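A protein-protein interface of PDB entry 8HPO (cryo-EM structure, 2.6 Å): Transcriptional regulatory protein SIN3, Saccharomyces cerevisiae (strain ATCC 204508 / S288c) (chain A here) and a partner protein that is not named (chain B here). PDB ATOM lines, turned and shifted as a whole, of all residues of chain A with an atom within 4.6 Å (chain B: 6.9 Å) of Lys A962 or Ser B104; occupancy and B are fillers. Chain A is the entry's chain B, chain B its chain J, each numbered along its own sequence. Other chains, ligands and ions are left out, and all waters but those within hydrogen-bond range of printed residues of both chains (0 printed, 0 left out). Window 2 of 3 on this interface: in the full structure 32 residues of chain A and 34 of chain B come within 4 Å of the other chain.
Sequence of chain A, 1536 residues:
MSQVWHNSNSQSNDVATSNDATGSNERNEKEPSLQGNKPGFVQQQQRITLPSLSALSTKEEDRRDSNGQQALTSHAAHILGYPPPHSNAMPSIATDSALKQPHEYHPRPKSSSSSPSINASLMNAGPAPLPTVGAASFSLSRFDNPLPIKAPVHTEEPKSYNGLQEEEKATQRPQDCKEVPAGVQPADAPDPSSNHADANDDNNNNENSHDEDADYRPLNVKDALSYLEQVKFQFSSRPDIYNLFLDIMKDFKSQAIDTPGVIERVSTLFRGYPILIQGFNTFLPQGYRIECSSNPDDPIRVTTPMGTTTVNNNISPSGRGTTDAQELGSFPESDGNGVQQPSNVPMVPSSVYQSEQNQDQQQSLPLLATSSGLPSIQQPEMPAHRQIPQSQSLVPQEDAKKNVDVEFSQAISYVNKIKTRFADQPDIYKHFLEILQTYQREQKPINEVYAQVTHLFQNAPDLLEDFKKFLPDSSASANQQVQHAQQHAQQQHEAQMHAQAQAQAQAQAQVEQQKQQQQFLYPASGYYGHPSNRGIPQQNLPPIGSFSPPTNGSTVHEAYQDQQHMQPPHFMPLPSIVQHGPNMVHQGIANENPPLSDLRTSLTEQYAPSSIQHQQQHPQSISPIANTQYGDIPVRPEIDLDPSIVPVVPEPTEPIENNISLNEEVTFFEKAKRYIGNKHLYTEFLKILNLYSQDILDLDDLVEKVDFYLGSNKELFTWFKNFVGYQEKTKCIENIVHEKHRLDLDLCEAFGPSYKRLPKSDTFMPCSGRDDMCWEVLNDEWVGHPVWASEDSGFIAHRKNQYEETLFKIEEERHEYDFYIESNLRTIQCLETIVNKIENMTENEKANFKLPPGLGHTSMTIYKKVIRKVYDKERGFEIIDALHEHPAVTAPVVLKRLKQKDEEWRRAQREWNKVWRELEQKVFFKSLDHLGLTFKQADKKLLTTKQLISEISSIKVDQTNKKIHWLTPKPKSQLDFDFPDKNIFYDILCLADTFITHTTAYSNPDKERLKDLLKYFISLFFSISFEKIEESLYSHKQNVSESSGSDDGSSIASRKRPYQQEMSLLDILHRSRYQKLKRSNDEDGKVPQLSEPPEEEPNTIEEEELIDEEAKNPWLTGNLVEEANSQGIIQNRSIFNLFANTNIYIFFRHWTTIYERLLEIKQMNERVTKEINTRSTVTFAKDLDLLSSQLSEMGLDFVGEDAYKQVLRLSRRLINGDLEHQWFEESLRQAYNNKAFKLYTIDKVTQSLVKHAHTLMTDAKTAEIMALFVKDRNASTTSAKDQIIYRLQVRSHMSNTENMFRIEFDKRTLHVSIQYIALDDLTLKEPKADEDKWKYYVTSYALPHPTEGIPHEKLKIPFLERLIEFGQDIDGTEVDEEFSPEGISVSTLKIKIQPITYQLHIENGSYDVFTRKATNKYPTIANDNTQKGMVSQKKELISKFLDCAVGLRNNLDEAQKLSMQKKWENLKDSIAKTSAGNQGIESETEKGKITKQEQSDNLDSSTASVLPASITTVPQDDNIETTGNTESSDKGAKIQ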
ATOM      1  N   ASP A 958     -22.964  14.919  -8.360  1.00  0.00           N
ATOM      2  CA  ASP A 958     -23.583  14.216  -9.471  1.00  0.00           C
ATOM      3  C   ASP A 958     -24.877  14.894  -9.890  1.00  0.00           C
ATOM      4  O   ASP A 958     -25.224  14.868 -11.074  1.00  0.00           O
ATOM      5  CB  ASP A 958     -23.797  12.737  -9.153  1.00  0.00           C
ATOM      6  CG  ASP A 958     -24.994  12.489  -8.278  1.00  0.00           C
ATOM      7  OD1 ASP A 958     -25.788  11.600  -8.617  1.00  0.00           O
ATOM      8  OD2 ASP A 958     -25.135  13.147  -7.239  1.00  0.00           O
ATOM      9  N   GLN A 959     -25.567  15.570  -8.967  1.00  0.00           N
ATOM     10  CA  GLN A 959     -26.686  16.407  -9.377  1.00  0.00           C
ATOM     11  C   GLN A 959     -26.234  17.472 -10.367  1.00  0.00           C
ATOM     12  O   GLN A 959     -26.824  17.627 -11.441  1.00  0.00           O
ATOM     13  CB  GLN A 959     -27.338  17.048  -8.154  1.00  0.00           C
ATOM     14  CG  GLN A 959     -28.595  16.347  -7.690  1.00  0.00           C
ATOM     15  CD  GLN A 959     -29.075  16.857  -6.351  1.00  0.00           C
ATOM     16  OE1 GLN A 959     -28.295  17.387  -5.561  1.00  0.00           O
ATOM     17  NE2 GLN A 959     -30.365  16.702  -6.087  1.00  0.00           N
ATOM     18  N   THR A 960     -25.168  18.205 -10.036  1.00  0.00           N
ATOM     19  CA  THR A 960     -24.757  19.298 -10.910  1.00  0.00           C
ATOM     20  C   THR A 960     -24.143  18.817 -12.221  1.00  0.00           C
ATOM     21  O   THR A 960     -24.239  19.532 -13.221  1.00  0.00           O
ATOM     22  CB  THR A 960     -23.781  20.247 -10.206  1.00  0.00           C
ATOM     23  OG1 THR A 960     -23.320  21.232 -11.140  1.00  0.00           O
ATOM     24  CG2 THR A 960     -22.589  19.512  -9.676  1.00  0.00           C
ATOM     25  N   ASN A 961     -23.529  17.631 -12.267  1.00  0.00           N
ATOM     26  CA  ASN A 961     -22.978  17.196 -13.550  1.00  0.00           C
ATOM     27  C   ASN A 961     -24.051  16.537 -14.410  1.00  0.00           C
ATOM     28  O   ASN A 961     -23.975  16.575 -15.642  1.00  0.00           O
ATOM     29  CB  ASN A 961     -21.773  16.268 -13.355  1.00  0.00           C
ATOM     30  CG  ASN A 961     -22.067  15.086 -12.468  1.00  0.00           C
ATOM     31  OD1 ASN A 961     -23.084  14.413 -12.618  1.00  0.00           O
ATOM     32  ND2 ASN A 961     -21.161  14.814 -11.539  1.00  0.00           N
ATOM     33  N   LYS A 962     -25.069  15.935 -13.783  1.00  0.00           N
ATOM     34  CA  LYS A 962     -26.282  15.614 -14.523  1.00  0.00           C
ATOM     35  C   LYS A 962     -26.946  16.876 -15.049  1.00  0.00           C
ATOM     36  O   LYS A 962     -27.564  16.857 -16.117  1.00  0.00           O
ATOM     37  CB  LYS A 962     -27.259  14.843 -13.638  1.00  0.00           C
ATOM     38  CG  LYS A 962     -28.289  14.055 -14.415  1.00  0.00           C
ATOM     39  CD  LYS A 962     -28.802  12.880 -13.618  1.00  0.00           C
ATOM     40  CE  LYS A 962     -29.010  11.682 -14.516  1.00  0.00           C
ATOM     41  NZ  LYS A 962     -30.362  11.705 -15.140  1.00  0.00           N
ATOM     42  N   LYS A 963     -26.849  17.970 -14.294  1.00  0.00           N
ATOM     43  CA  LYS A 963     -27.338  19.262 -14.760  1.00  0.00           C
ATOM     44  C   LYS A 963     -26.544  19.748 -15.967  1.00  0.00           C
ATOM     45  O   LYS A 963     -27.116  20.317 -16.904  1.00  0.00           O
ATOM     46  CB  LYS A 963     -27.258  20.274 -13.620  1.00  0.00           C
ATOM     47  CG  LYS A 963     -27.931  21.597 -13.883  1.00  0.00           C
ATOM     48  CD  LYS A 963     -27.427  22.648 -12.905  1.00  0.00           C
ATOM     49  CE  LYS A 963     -27.246  22.074 -11.509  1.00  0.00           C
ATOM     50  NZ  LYS A 963     -26.985  23.128 -10.491  1.00  0.00           N
ATOM     51  N   ILE A 964     -25.224  19.548 -15.951  1.00  0.00           N
ATOM     52  CA  ILE A 964     -24.408  19.874 -17.117  1.00  0.00           C
ATOM     53  C   ILE A 964     -24.919  19.127 -18.340  1.00  0.00           C
ATOM     54  O   ILE A 964     -24.858  19.631 -19.469  1.00  0.00           O
ATOM     55  CB  ILE A 964     -22.925  19.569 -16.836  1.00  0.00           C
ATOM     56  CG1 ILE A 964     -22.416  20.415 -15.667  1.00  0.00           C
ATOM     57  CG2 ILE A 964     -22.075  19.820 -18.068  1.00  0.00           C
ATOM     58  CD1 ILE A 964     -22.776  21.884 -15.758  1.00  0.00           C
ATOM     59  N   HIS A 965     -25.440  17.921 -18.139  1.00  0.00           N
ATOM     60  CA  HIS A 965     -26.177  17.254 -19.200  1.00  0.00           C
ATOM     61  C   HIS A 965     -27.557  17.880 -19.321  1.00  0.00           C
ATOM     62  O   HIS A 965     -28.198  18.204 -18.317  1.00  0.00           O
ATOM     63  CB  HIS A 965     -26.290  15.757 -18.924  1.00  0.00           C
ATOM     64  CG  HIS A 965     -26.598  14.947 -20.144  1.00  0.00           C
ATOM     65  ND1 HIS A 965     -26.692  13.572 -20.122  1.00  0.00           N
ATOM     66  CD2 HIS A 965     -26.832  15.321 -21.424  1.00  0.00           C
ATOM     67  CE1 HIS A 965     -26.966  13.134 -21.338  1.00  0.00           C
ATOM     68  NE2 HIS A 965     -27.060  14.174 -22.146  1.00  0.00           N
ATOM     69  N   THR A 968     -31.874  16.557 -17.331  1.00  0.00           N
ATOM     70  CA  THR A 968     -32.649  17.027 -16.191  1.00  0.00           C
ATOM     71  C   THR A 968     -32.583  18.546 -16.115  1.00  0.00           C
ATOM     72  O   THR A 968     -31.541  19.127 -16.456  1.00  0.00           O
ATOM     73  CB  THR A 968     -32.135  16.417 -14.893  1.00  0.00           C
ATOM     74  OG1 THR A 968     -32.732  17.095 -13.781  1.00  0.00           O
ATOM     75  CG2 THR A 968     -30.638  16.572 -14.806  1.00  0.00           C
ATOM     76  N   ASN B  93     -18.616   9.011 -14.971  1.00  0.00           N
ATOM     77  CA  ASN B  93     -19.123   9.131 -13.616  1.00  0.00           C
ATOM     78  C   ASN B  93     -17.931   8.950 -12.694  1.00  0.00           C
ATOM     79  O   ASN B  93     -16.910   8.391 -13.101  1.00  0.00           O
ATOM     80  CB  ASN B  93     -20.212   8.091 -13.328  1.00  0.00           C
ATOM     81  CG  ASN B  93     -20.840   8.256 -11.958  1.00  0.00           C
ATOM     82  OD1 ASN B  93     -20.158   8.511 -10.967  1.00  0.00           O
ATOM     83  ND2 ASN B  93     -22.155   8.110 -11.898  1.00  0.00           N
ATOM     84  N   LYS B  96     -19.183   5.348  -9.901  1.00  0.00           N
ATOM     85  CA  LYS B  96     -19.808   4.141 -10.408  1.00  0.00           C
ATOM     86  C   LYS B  96     -19.158   3.767 -11.731  1.00  0.00           C
ATOM     87  O   LYS B  96     -18.088   4.268 -12.085  1.00  0.00           O
ATOM     88  CB  LYS B  96     -21.313   4.337 -10.607  1.00  0.00           C
ATOM     89  CG  LYS B  96     -22.167   4.332  -9.364  1.00  0.00           C
ATOM     90  CD  LYS B  96     -23.564   4.832  -9.706  1.00  0.00           C
ATOM     91  CE  LYS B  96     -24.136   4.112 -10.930  1.00  0.00           C
ATOM     92  NZ  LYS B  96     -23.900   4.821 -12.227  1.00  0.00           N
ATOM     93  N   ASP B 101     -25.689   2.006 -22.652  1.00  0.00           N
ATOM     94  CA  ASP B 101     -26.958   2.702 -22.832  1.00  0.00           C
ATOM     95  C   ASP B 101     -27.091   3.859 -21.852  1.00  0.00           C
ATOM     96  O   ASP B 101     -27.823   4.817 -22.118  1.00  0.00           O
ATOM     97  CB  ASP B 101     -28.130   1.728 -22.685  1.00  0.00           C
ATOM     98  CG  ASP B 101     -28.058   0.901 -21.410  1.00  0.00           C
ATOM     99  OD1 ASP B 101     -27.295   1.263 -20.488  1.00  0.00           O
ATOM    100  OD2 ASP B 101     -28.782  -0.113 -21.324  1.00  0.00           O
ATOM    101  N   GLU B 102     -26.390   3.771 -20.721  1.00  0.00           N
ATOM    102  CA  GLU B 102     -26.288   4.841 -19.733  1.00  0.00           C
ATOM    103  C   GLU B 102     -27.666   5.259 -19.215  1.00  0.00           C
ATOM    104  O   GLU B 102     -28.156   6.363 -19.465  1.00  0.00           O
ATOM    105  CB  GLU B 102     -25.523   6.048 -20.286  1.00  0.00           C
ATOM    106  CG  GLU B 102     -24.938   6.944 -19.197  1.00  0.00           C
ATOM    107  CD  GLU B 102     -23.865   6.254 -18.372  1.00  0.00           C
ATOM    108  OE1 GLU B 102     -22.671   6.378 -18.720  1.00  0.00           O
ATOM    109  OE2 GLU B 102     -24.212   5.595 -17.368  1.00  0.00           O
ATOM    110  N   ASP B 103     -28.290   4.327 -18.498  1.00  0.00           N
ATOM    111  CA  ASP B 103     -29.354   4.720 -17.585  1.00  0.00           C
ATOM    112  C   ASP B 103     -28.794   5.787 -16.653  1.00  0.00           C
ATOM    113  O   ASP B 103     -27.581   5.824 -16.410  1.00  0.00           O
ATOM    114  CB  ASP B 103     -29.886   3.525 -16.791  1.00  0.00           C
ATOM    115  CG  ASP B 103     -28.848   2.934 -15.857  1.00  0.00           C
ATOM    116  OD1 ASP B 103     -28.663   3.486 -14.751  1.00  0.00           O
ATOM    117  OD2 ASP B 103     -28.224   1.917 -16.227  1.00  0.00           O
ATOM    118  N   SER B 104     -29.665   6.653 -16.138  1.00  0.00           N
ATOM    119  CA  SER B 104     -29.228   7.832 -15.400  1.00  0.00           C
ATOM    120  C   SER B 104     -28.201   7.473 -14.330  1.00  0.00           C
ATOM    121  O   SER B 104     -28.284   6.410 -13.706  1.00  0.00           O
ATOM    122  CB  SER B 104     -30.438   8.521 -14.783  1.00  0.00           C
ATOM    123  OG  SER B 104     -31.258   9.101 -15.785  1.00  0.00           O
ATOM    124  N   THR B 105     -27.222   8.359 -14.138  1.00  0.00           N
ATOM    125  CA  THR B 105     -26.020   8.007 -13.390  1.00  0.00           C
ATOM    126  C   THR B 105     -26.332   7.674 -11.935  1.00  0.00           C
ATOM    127  O   THR B 105     -25.866   6.660 -11.408  1.00  0.00           O
ATOM    128  CB  THR B 105     -25.000   9.142 -13.475  1.00  0.00           C
ATOM    129  OG1 THR B 105     -25.353  10.177 -12.551  1.00  0.00           O
ATOM    130  CG2 THR B 105     -24.971   9.708 -14.870  1.00  0.00           C
ATOM    131  N   SER B 106     -27.120   8.514 -11.267  1.00  0.00           N
ATOM    132  CA  SER B 106     -27.371   8.333  -9.840  1.00  0.00           C
ATOM    133  C   SER B 106     -28.348   7.211  -9.530  1.00  0.00           C
ATOM    134  O   SER B 106     -28.776   7.100  -8.375  1.00  0.00           O
ATOM    135  CB  SER B 106     -27.905   9.627  -9.236  1.00  0.00           C
ATOM    136  OG  SER B 106     -27.478   9.751  -7.892  1.00  0.00           O
ATOM    137  N   TYR B 107     -28.716   6.398 -10.520  1.00  0.00           N
ATOM    138  CA  TYR B 107     -29.824   5.465 -10.346  1.00  0.00           C
ATOM    139  C   TYR B 107     -29.608   4.528  -9.163  1.00  0.00           C
ATOM    140  O   TYR B 107     -30.470   4.429  -8.282  1.00  0.00           O
ATOM    141  CB  TYR B 107     -30.038   4.679 -11.638  1.00  0.00           C
ATOM    142  CG  TYR B 107     -31.105   5.277 -12.514  1.00  0.00           C
ATOM    143  CD1 TYR B 107     -31.730   6.461 -12.158  1.00  0.00           C
ATOM    144  CD2 TYR B 107     -31.468   4.681 -13.715  1.00  0.00           C
ATOM    145  CE1 TYR B 107     -32.715   7.013 -12.950  1.00  0.00           C
ATOM    146  CE2 TYR B 107     -32.442   5.233 -14.520  1.00  0.00           C
ATOM    147  CZ  TYR B 107     -33.066   6.395 -14.131  1.00  0.00           C
ATOM    148  OH  TYR B 107     -34.032   6.957 -14.928  1.00  0.00           O
ATOM    149  N   SER B 108     -28.476   3.836  -9.117  1.00  0.00           N
ATOM    150  CA  SER B 108     -28.247   2.825  -8.089  1.00  0.00           C
ATOM    151  C   SER B 108     -27.380   3.406  -6.976  1.00  0.00           C
ATOM    152  O   SER B 108     -26.324   3.990  -7.239  1.00  0.00           O
ATOM    153  CB  SER B 108     -27.603   1.578  -8.686  1.00  0.00           C
ATOM    154  OG  SER B 108     -26.974   0.811  -7.675  1.00  0.00           O
ATOM    155  N   GLU B 146     -15.986  20.179 -14.235  1.00  0.00           N
ATOM    156  CA  GLU B 146     -15.837  20.005 -12.795  1.00  0.00           C
ATOM    157  C   GLU B 146     -15.154  18.690 -12.452  1.00  0.00           C
ATOM    158  O   GLU B 146     -14.428  18.615 -11.459  1.00  0.00           O
ATOM    159  CB  GLU B 146     -17.199  20.097 -12.112  1.00  0.00           C
ATOM    160  CG  GLU B 146     -18.342  19.553 -12.945  1.00  0.00           C
ATOM    161  CD  GLU B 146     -19.127  20.652 -13.632  1.00  0.00           C
ATOM    162  OE1 GLU B 146     -18.554  21.330 -14.508  1.00  0.00           O
ATOM    163  OE2 GLU B 146     -20.312  20.846 -13.292  1.00  0.00           O
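OG of Ser B104 sits at hydrogen-bond distance from NZ of Lys A962, 2.8 Å away. The side-chain carboxylate (OD1) of Asp A958 is in hydrogen-bond range of the side-chain hydroxyl (OG) of Ser B106 (2.6 Å).
NZ of Lys B96 lies within hydrogen-bond range of O of Thr B105, 2.8 Å away. The backbone carbonyl oxygen (O) of Asp A958 lies close to the side-chain amide oxygen (OD1) of Asn A961, 2.7 Å away.
Thr A960 touches Glu B146. Thr B105 touches Lys A962. Ile A964 touches Glu B146 (CG1 to OE2, 3.2 Å).
Printed residues of chain B within 4 Å of Asp A958: Ser B106. Of the printed residues of chain B, Thr A960 touches Glu B146 (3.7 Å). Asn A961 touches none of the printed residues of chain B. Lys A962 touches just these residues of chain B: Ser B104 and Thr B105. Printed residues of chain B within 4 Å of Ile A964: Glu B146. Ser B104 touches one residue of chain A. Printed residues of chain A within 4 Å of Thr B105: Lys A962 (3.8 Å). Printed residues of chain A within 4 Å of Ser B106: Asp A958. The nearest printed residue of chain A that does not touch Ser B104 is Thr A968 (7.4 Å). The nearest printed residue of chain B that does not touch Asp A958 is Thr B105 (4.2 Å).
Hydrophobic or aromatic side chains of chain A within 4 Å of the printed part of chain B: Ile A964. Among the printed residues, 5 pairs touch across the chains. Among the printed residues, no Asp or Glu carboxylate lies within 4 Å of a Lys or Arg side-chain nitrogen of the other chain.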
